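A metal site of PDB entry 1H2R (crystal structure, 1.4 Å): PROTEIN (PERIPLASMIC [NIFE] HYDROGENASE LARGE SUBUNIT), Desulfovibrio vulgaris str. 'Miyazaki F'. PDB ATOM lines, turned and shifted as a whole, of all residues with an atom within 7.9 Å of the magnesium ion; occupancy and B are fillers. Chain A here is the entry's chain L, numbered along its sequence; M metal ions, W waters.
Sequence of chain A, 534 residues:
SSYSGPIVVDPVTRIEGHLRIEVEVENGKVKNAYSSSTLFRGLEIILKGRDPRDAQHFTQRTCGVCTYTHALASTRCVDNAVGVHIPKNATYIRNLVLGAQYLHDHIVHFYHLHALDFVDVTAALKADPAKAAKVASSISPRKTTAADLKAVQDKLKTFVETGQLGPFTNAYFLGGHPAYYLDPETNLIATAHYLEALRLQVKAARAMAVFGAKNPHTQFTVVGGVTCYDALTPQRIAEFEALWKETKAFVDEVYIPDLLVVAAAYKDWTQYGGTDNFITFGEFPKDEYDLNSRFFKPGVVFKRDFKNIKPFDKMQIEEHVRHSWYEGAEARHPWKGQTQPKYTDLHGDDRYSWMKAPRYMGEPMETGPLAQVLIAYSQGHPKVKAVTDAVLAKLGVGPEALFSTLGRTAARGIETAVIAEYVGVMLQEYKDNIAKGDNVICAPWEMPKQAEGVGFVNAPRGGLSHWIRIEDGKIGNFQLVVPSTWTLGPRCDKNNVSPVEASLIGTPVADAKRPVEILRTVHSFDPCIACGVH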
ATOM      1  N   GLU A  44       3.464  -9.562   0.342  1.00  0.00           N
ATOM      2  CA  GLU A  44       3.996  -8.229   0.048  1.00  0.00           C
ATOM      3  C   GLU A  44       4.917  -8.240  -1.183  1.00  0.00           C
ATOM      4  O   GLU A  44       4.902  -7.298  -1.977  1.00  0.00           O
ATOM      5  CB  GLU A  44       4.726  -7.647   1.264  1.00  0.00           C
ATOM      6  CG  GLU A  44       3.827  -7.353   2.470  1.00  0.00           C
ATOM      7  CD  GLU A  44       4.550  -7.478   3.810  1.00  0.00           C
ATOM      8  OE1 GLU A  44       5.600  -8.179   3.847  1.00  0.00           O
ATOM      9  OE2 GLU A  44       4.069  -6.873   4.814  1.00  0.00           O
ATOM     10  N   GLU A 319       9.370  -1.978  12.168  1.00  0.00           N
ATOM     11  CA  GLU A 319       9.416  -3.430  12.219  1.00  0.00           C
ATOM     12  C   GLU A 319      10.851  -3.934  12.118  1.00  0.00           C
ATOM     13  O   GLU A 319      11.547  -3.666  11.131  1.00  0.00           O
ATOM     14  CB  GLU A 319       8.576  -4.046  11.093  1.00  0.00           C
ATOM     15  CG  GLU A 319       7.107  -3.717  11.164  1.00  0.00           C
ATOM     16  CD  GLU A 319       6.336  -4.502  10.140  1.00  0.00           C
ATOM     17  OE1 GLU A 319       5.759  -5.536  10.499  1.00  0.00           O
ATOM     18  OE2 GLU A 319       6.327  -4.079   8.966  1.00  0.00           O
ATOM     19  N   TYR A 326      15.096 -12.650   7.705  1.00  0.00           N
ATOM     20  CA  TYR A 326      15.152 -11.678   6.624  1.00  0.00           C
ATOM     21  C   TYR A 326      16.589 -11.144   6.580  1.00  0.00           C
ATOM     22  O   TYR A 326      17.339 -11.299   7.532  1.00  0.00           O
ATOM     23  CB  TYR A 326      14.150 -10.532   6.863  1.00  0.00           C
ATOM     24  CG  TYR A 326      12.693 -10.994   6.876  1.00  0.00           C
ATOM     25  CD1 TYR A 326      12.006 -11.193   8.082  1.00  0.00           C
ATOM     26  CD2 TYR A 326      12.028 -11.278   5.690  1.00  0.00           C
ATOM     27  CE1 TYR A 326      10.692 -11.679   8.102  1.00  0.00           C
ATOM     28  CE2 TYR A 326      10.722 -11.760   5.687  1.00  0.00           C
ATOM     29  CZ  TYR A 326      10.059 -11.966   6.892  1.00  0.00           C
ATOM     30  OH  TYR A 326       8.770 -12.478   6.848  1.00  0.00           O
ATOM     31  N   PRO A 334       6.894   1.066   7.962  1.00  0.00           N
ATOM     32  CA  PRO A 334       6.130   0.458   6.852  1.00  0.00           C
ATOM     33  C   PRO A 334       6.148   1.159   5.463  1.00  0.00           C
ATOM     34  O   PRO A 334       6.071   0.496   4.427  1.00  0.00           O
ATOM     35  CB  PRO A 334       4.720   0.358   7.424  1.00  0.00           C
ATOM     36  CG  PRO A 334       4.951   0.170   8.884  1.00  0.00           C
ATOM     37  CD  PRO A 334       6.053   1.151   9.177  1.00  0.00           C
ATOM     38  N   GLN A 338      10.746  -3.426   3.943  1.00  0.00           N
ATOM     39  CA  GLN A 338      11.487  -4.389   3.138  1.00  0.00           C
ATOM     40  C   GLN A 338      11.090  -5.816   3.531  1.00  0.00           C
ATOM     41  O   GLN A 338      10.966  -6.125   4.705  1.00  0.00           O
ATOM     42  CB  GLN A 338      12.994  -4.239   3.361  1.00  0.00           C
ATOM     43  CG  GLN A 338      13.586  -2.920   2.917  1.00  0.00           C
ATOM     44  CD  GLN A 338      15.079  -2.896   3.114  1.00  0.00           C
ATOM     45  OE1 GLN A 338      15.844  -2.800   2.149  1.00  0.00           O
ATOM     46  NE2 GLN A 338      15.524  -3.007   4.356  1.00  0.00           N
ATOM     47  N   THR A 339      10.921  -6.684   2.539  1.00  0.00           N
ATOM     48  CA  THR A 339      10.579  -8.076   2.805  1.00  0.00           C
ATOM     49  C   THR A 339      11.523  -8.914   1.944  1.00  0.00           C
ATOM     50  O   THR A 339      11.223  -9.260   0.793  1.00  0.00           O
ATOM     51  CB  THR A 339       9.081  -8.350   2.521  1.00  0.00           C
ATOM     52  OG1 THR A 339       8.312  -7.386   3.240  1.00  0.00           O
ATOM     53  CG2 THR A 339       8.687  -9.735   3.014  1.00  0.00           C
ATOM     54  N   TRP A 354       9.514 -16.236  11.171  1.00  0.00           N
ATOM     55  CA  TRP A 354       9.225 -15.577   9.895  1.00  0.00           C
ATOM     56  C   TRP A 354       8.463 -14.280  10.173  1.00  0.00           C
ATOM     57  O   TRP A 354       8.209 -13.493   9.260  1.00  0.00           O
ATOM     58  CB  TRP A 354       8.423 -16.490   8.954  1.00  0.00           C
ATOM     59  CG  TRP A 354       9.269 -17.512   8.241  1.00  0.00           C
ATOM     60  CD1 TRP A 354       9.223 -18.859   8.412  1.00  0.00           C
ATOM     61  CD2 TRP A 354      10.270 -17.272   7.227  1.00  0.00           C
ATOM     62  NE1 TRP A 354      10.120 -19.477   7.571  1.00  0.00           N
ATOM     63  CE2 TRP A 354      10.781 -18.533   6.834  1.00  0.00           C
ATOM     64  CE3 TRP A 354      10.779 -16.113   6.622  1.00  0.00           C
ATOM     65  CZ2 TRP A 354      11.792 -18.671   5.861  1.00  0.00           C
ATOM     66  CZ3 TRP A 354      11.767 -16.245   5.650  1.00  0.00           C
ATOM     67  CH2 TRP A 354      12.271 -17.520   5.283  1.00  0.00           C
ATOM     68  N   MET A 355       8.092 -14.066  11.430  1.00  0.00           N
ATOM     69  CA  MET A 355       7.400 -12.828  11.786  1.00  0.00           C
ATOM     70  C   MET A 355       8.429 -11.704  12.005  1.00  0.00           C
ATOM     71  O   MET A 355       9.506 -11.972  12.569  1.00  0.00           O
ATOM     72  CB  MET A 355       6.591 -12.966  13.090  1.00  0.00           C
ATOM     73  CG  MET A 355       5.188 -13.549  12.953  1.00  0.00           C
ATOM     74  SD  MET A 355       4.103 -13.066  14.330  1.00  0.00           S
ATOM     75  CE  MET A 355       2.979 -14.445  14.548  1.00  0.00           C
ATOM     76  N   LYS A 356       8.107 -10.496  11.565  1.00  0.00           N
ATOM     77  CA  LYS A 356       8.946  -9.318  11.828  1.00  0.00           C
ATOM     78  C   LYS A 356       8.569  -8.912  13.260  1.00  0.00           C
ATOM     79  O   LYS A 356       7.562  -9.403  13.810  1.00  0.00           O
ATOM     80  CB  LYS A 356       8.598  -8.175  10.883  1.00  0.00           C
ATOM     81  CG  LYS A 356       9.040  -8.401   9.440  1.00  0.00           C
ATOM     82  CD  LYS A 356       8.678  -7.221   8.556  1.00  0.00           C
ATOM     83  CE  LYS A 356       9.193  -7.420   7.124  1.00  0.00           C
ATOM     84  NZ  LYS A 356       8.494  -6.510   6.183  1.00  0.00           N
ATOM     85  N   PRO A 358       7.420  -5.744  15.358  1.00  0.00           N
ATOM     86  CA  PRO A 358       6.987  -4.340  15.448  1.00  0.00           C
ATOM     87  C   PRO A 358       7.226  -3.780  16.848  1.00  0.00           C
ATOM     88  O   PRO A 358       6.945  -4.443  17.860  1.00  0.00           O
ATOM     89  CB  PRO A 358       5.468  -4.419  15.188  1.00  0.00           C
ATOM     90  CG  PRO A 358       5.272  -5.701  14.487  1.00  0.00           C
ATOM     91  CD  PRO A 358       6.272  -6.638  15.131  1.00  0.00           C
ATOM     92  N   SER A 465      -2.943  -2.470  10.332  1.00  0.00           N
ATOM     93  CA  SER A 465      -2.647  -1.370   9.422  1.00  0.00           C
ATOM     94  C   SER A 465      -1.991  -1.846   8.111  1.00  0.00           C
ATOM     95  O   SER A 465      -1.131  -2.736   8.127  1.00  0.00           O
ATOM     96  CB  SER A 465      -1.764  -0.317  10.113  1.00  0.00           C
ATOM     97  OG  SER A 465      -0.537  -0.868  10.565  1.00  0.00           O
ATOM     98  N   TRP A 467      -0.188  -0.380   4.506  1.00  0.00           N
ATOM     99  CA  TRP A 467       0.545   0.810   4.007  1.00  0.00           C
ATOM    100  C   TRP A 467       0.958   0.697   2.536  1.00  0.00           C
ATOM    101  O   TRP A 467       1.651  -0.254   2.143  1.00  0.00           O
ATOM    102  CB  TRP A 467       1.810   1.012   4.848  1.00  0.00           C
ATOM    103  CG  TRP A 467       1.590   0.995   6.333  1.00  0.00           C
ATOM    104  CD1 TRP A 467       1.307  -0.086   7.128  1.00  0.00           C
ATOM    105  CD2 TRP A 467       1.654   2.129   7.219  1.00  0.00           C
ATOM    106  NE1 TRP A 467       1.206   0.302   8.444  1.00  0.00           N
ATOM    107  CE2 TRP A 467       1.409   1.649   8.527  1.00  0.00           C
ATOM    108  CE3 TRP A 467       1.899   3.505   7.026  1.00  0.00           C
ATOM    109  CZ2 TRP A 467       1.396   2.501   9.644  1.00  0.00           C
ATOM    110  CZ3 TRP A 467       1.889   4.343   8.132  1.00  0.00           C
ATOM    111  CH2 TRP A 467       1.645   3.828   9.427  1.00  0.00           C
ATOM    112  N   PHE A 478       3.994  -2.243  -0.721  1.00  0.00           N
ATOM    113  CA  PHE A 478       2.777  -2.523   0.049  1.00  0.00           C
ATOM    114  C   PHE A 478       3.226  -3.357   1.249  1.00  0.00           C
ATOM    115  O   PHE A 478       3.813  -4.431   1.105  1.00  0.00           O
ATOM    116  CB  PHE A 478       1.726  -3.299  -0.783  1.00  0.00           C
ATOM    117  CG  PHE A 478       0.302  -3.147  -0.247  1.00  0.00           C
ATOM    118  CD1 PHE A 478      -0.108  -3.810   0.909  1.00  0.00           C
ATOM    119  CD2 PHE A 478      -0.608  -2.298  -0.883  1.00  0.00           C
ATOM    120  CE1 PHE A 478      -1.413  -3.630   1.433  1.00  0.00           C
ATOM    121  CE2 PHE A 478      -1.911  -2.121  -0.372  1.00  0.00           C
ATOM    122  CZ  PHE A 478      -2.305  -2.791   0.788  1.00  0.00           C
ATOM    123  N   GLN A 479       2.921  -2.843   2.439  1.00  0.00           N
ATOM    124  CA  GLN A 479       3.312  -3.519   3.668  1.00  0.00           C
ATOM    125  C   GLN A 479       2.151  -3.671   4.649  1.00  0.00           C
ATOM    126  O   GLN A 479       1.376  -2.729   4.853  1.00  0.00           O
ATOM    127  CB  GLN A 479       4.433  -2.726   4.342  1.00  0.00           C
ATOM    128  CG  GLN A 479       5.734  -2.603   3.562  1.00  0.00           C
ATOM    129  CD  GLN A 479       6.557  -3.873   3.576  1.00  0.00           C
ATOM    130  OE1 GLN A 479       6.583  -4.604   4.565  1.00  0.00           O
ATOM    131  NE2 GLN A 479       7.246  -4.142   2.472  1.00  0.00           N
ATOM    132  N   LEU A 480       2.029  -4.866   5.218  1.00  0.00           N
ATOM    133  CA  LEU A 480       1.005  -5.167   6.224  1.00  0.00           C
ATOM    134  C   LEU A 480       1.680  -5.315   7.585  1.00  0.00           C
ATOM    135  O   LEU A 480       2.723  -5.970   7.674  1.00  0.00           O
ATOM    136  CB  LEU A 480       0.299  -6.511   5.931  1.00  0.00           C
ATOM    137  CG  LEU A 480      -0.610  -6.658   4.714  1.00  0.00           C
ATOM    138  CD1 LEU A 480       0.217  -6.760   3.450  1.00  0.00           C
ATOM    139  CD2 LEU A 480      -1.446  -7.924   4.854  1.00  0.00           C
ATOM    140  N   VAL A 481       1.087  -4.704   8.608  1.00  0.00           N
ATOM    141  CA  VAL A 481       1.556  -4.792  10.010  1.00  0.00           C
ATOM    142  C   VAL A 481       0.291  -5.240  10.746  1.00  0.00           C
ATOM    143  O   VAL A 481      -0.642  -4.437  10.936  1.00  0.00           O
ATOM    144  CB  VAL A 481       2.038  -3.433  10.584  1.00  0.00           C
ATOM    145  CG1 VAL A 481       2.614  -3.645  11.970  1.00  0.00           C
ATOM    146  CG2 VAL A 481       3.068  -2.799   9.694  1.00  0.00           C
ATOM    147  N   VAL A 482       0.240  -6.500  11.166  1.00  0.00           N
ATOM    148  CA  VAL A 482      -0.980  -7.034  11.770  1.00  0.00           C
ATOM    149  C   VAL A 482      -0.912  -7.292  13.270  1.00  0.00           C
ATOM    150  O   VAL A 482       0.169  -7.469  13.818  1.00  0.00           O
ATOM    151  CB  VAL A 482      -1.523  -8.269  10.944  1.00  0.00           C
ATOM    152  CG1 VAL A 482      -0.751  -8.428   9.628  1.00  0.00           C
ATOM    153  CG2 VAL A 482      -1.549  -9.541  11.757  1.00  0.00           C
ATOM    154  N   THR A 485       1.386  -9.927  14.707  1.00  0.00           N
ATOM    155  CA  THR A 485       2.811  -9.605  14.499  1.00  0.00           C
ATOM    156  C   THR A 485       3.246  -8.850  15.763  1.00  0.00           C
ATOM    157  O   THR A 485       4.292  -9.142  16.337  1.00  0.00           O
ATOM    158  CB  THR A 485       3.057  -8.679  13.259  1.00  0.00           C
ATOM    159  OG1 THR A 485       2.241  -9.106  12.149  1.00  0.00           O
ATOM    160  CG2 THR A 485       4.532  -8.766  12.801  1.00  0.00           C
ATOM    161  N   CYS A 531      -1.899 -14.404   9.626  1.00  0.00           N
ATOM    162  CA  CYS A 531      -1.991 -12.961   9.779  1.00  0.00           C
ATOM    163  C   CYS A 531      -0.604 -12.385  10.109  1.00  0.00           C
ATOM    164  O   CYS A 531      -0.137 -11.478   9.435  1.00  0.00           O
ATOM    165  CB  CYS A 531      -2.958 -12.592  10.924  1.00  0.00           C
ATOM    166  SG  CYS A 531      -4.655 -12.216  10.384  1.00  0.00           S
ATOM    167  N   GLY A 532       0.024 -12.903  11.159  1.00  0.00           N
ATOM    168  CA  GLY A 532       1.328 -12.388  11.582  1.00  0.00           C
ATOM    169  C   GLY A 532       2.477 -12.341  10.578  1.00  0.00           C
ATOM    170  O   GLY A 532       3.276 -11.384  10.593  1.00  0.00           O
ATOM    171  N   VAL A 533       2.595 -13.364   9.740  1.00  0.00           N
ATOM    172  CA  VAL A 533       3.677 -13.418   8.754  1.00  0.00           C
ATOM    173  C   VAL A 533       3.311 -12.953   7.343  1.00  0.00           C
ATOM    174  O   VAL A 533       4.085 -12.219   6.719  1.00  0.00           O
ATOM    175  CB  VAL A 533       4.235 -14.873   8.601  1.00  0.00           C
ATOM    176  CG1 VAL A 533       5.381 -14.899   7.565  1.00  0.00           C
ATOM    177  CG2 VAL A 533       4.716 -15.409   9.953  1.00  0.00           C
ATOM    178  N   HIS A 534       2.137 -13.376   6.868  1.00  0.00           N
ATOM    179  CA  HIS A 534       1.677 -13.071   5.510  1.00  0.00           C
ATOM    180  C   HIS A 534       2.756 -13.380   4.425  1.00  0.00           C
ATOM    181  O   HIS A 534       3.402 -14.444   4.554  1.00  0.00           O
ATOM    182  CB  HIS A 534       1.040 -11.674   5.385  1.00  0.00           C
ATOM    183  CG  HIS A 534       1.760 -10.599   6.142  1.00  0.00           C
ATOM    184  ND1 HIS A 534       1.598 -10.351   7.488  1.00  0.00           N
ATOM    185  CD2 HIS A 534       2.643  -9.670   5.710  1.00  0.00           C
ATOM    186  CE1 HIS A 534       2.366  -9.314   7.818  1.00  0.00           C
ATOM    187  NE2 HIS A 534       3.021  -8.861   6.765  1.00  0.00           N
ATOM    188  OXT HIS A 534       2.963 -12.596   3.471  1.00  0.00           O
HETATM  189 MG    MG M   1       4.408  -7.189   6.966  1.00  0.00          MG
HETATM  190  O   HOH W   1       5.649  -5.526   6.946  1.00  0.00           O
HETATM  191  O   HOH W   2       6.075  -8.381   6.462  1.00  0.00           O
HETATM  192  O   HOH W   3       4.829  -7.465   8.992  1.00  0.00           O
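Within 4 Å of the magnesium ion: Glu 44, Leu 480 and His 534. The nearest printed residue that does not touch the magnesium ion is Glu 319 (4.1 Å).
The magnesium ion is bound by water W1 (2.1 Å). Water W3 binds the magnesium ion (2.1 Å). Water W2 binds the magnesium ion, at 2.1 Å. NE2 of His 534 is bound to the magnesium ion. The magnesium ion is bound by O of Leu 480. The magnesium ion is bound by OE2 of Glu 44. The magnesium ion has six donor atoms within binding distance.
A ring nitrogen (ND1) of His 534 sits at hydrogen-bond distance from the backbone carbonyl oxygen (O) of Cys 531 (2.8 Å). OE2 of Glu 44 sits close to OE1 of Gln 479, 3.4 Å away. The side-chain hydroxyl of Thr 339 sits at hydrogen-bond distance from the side-chain carboxylate of Glu 44 (2.9 Å).
Water W2 bridges the side-chain carboxylate of Glu 44 and the side-chain amino group of Lys 356. Water W1 lies within hydrogen-bond range of the side-chain carboxylate of Glu 319 (2.6 Å), the side-chain amide oxygen of Gln 479 (2.7 Å) and the side-chain amino group of Lys 356 (3.1 Å).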
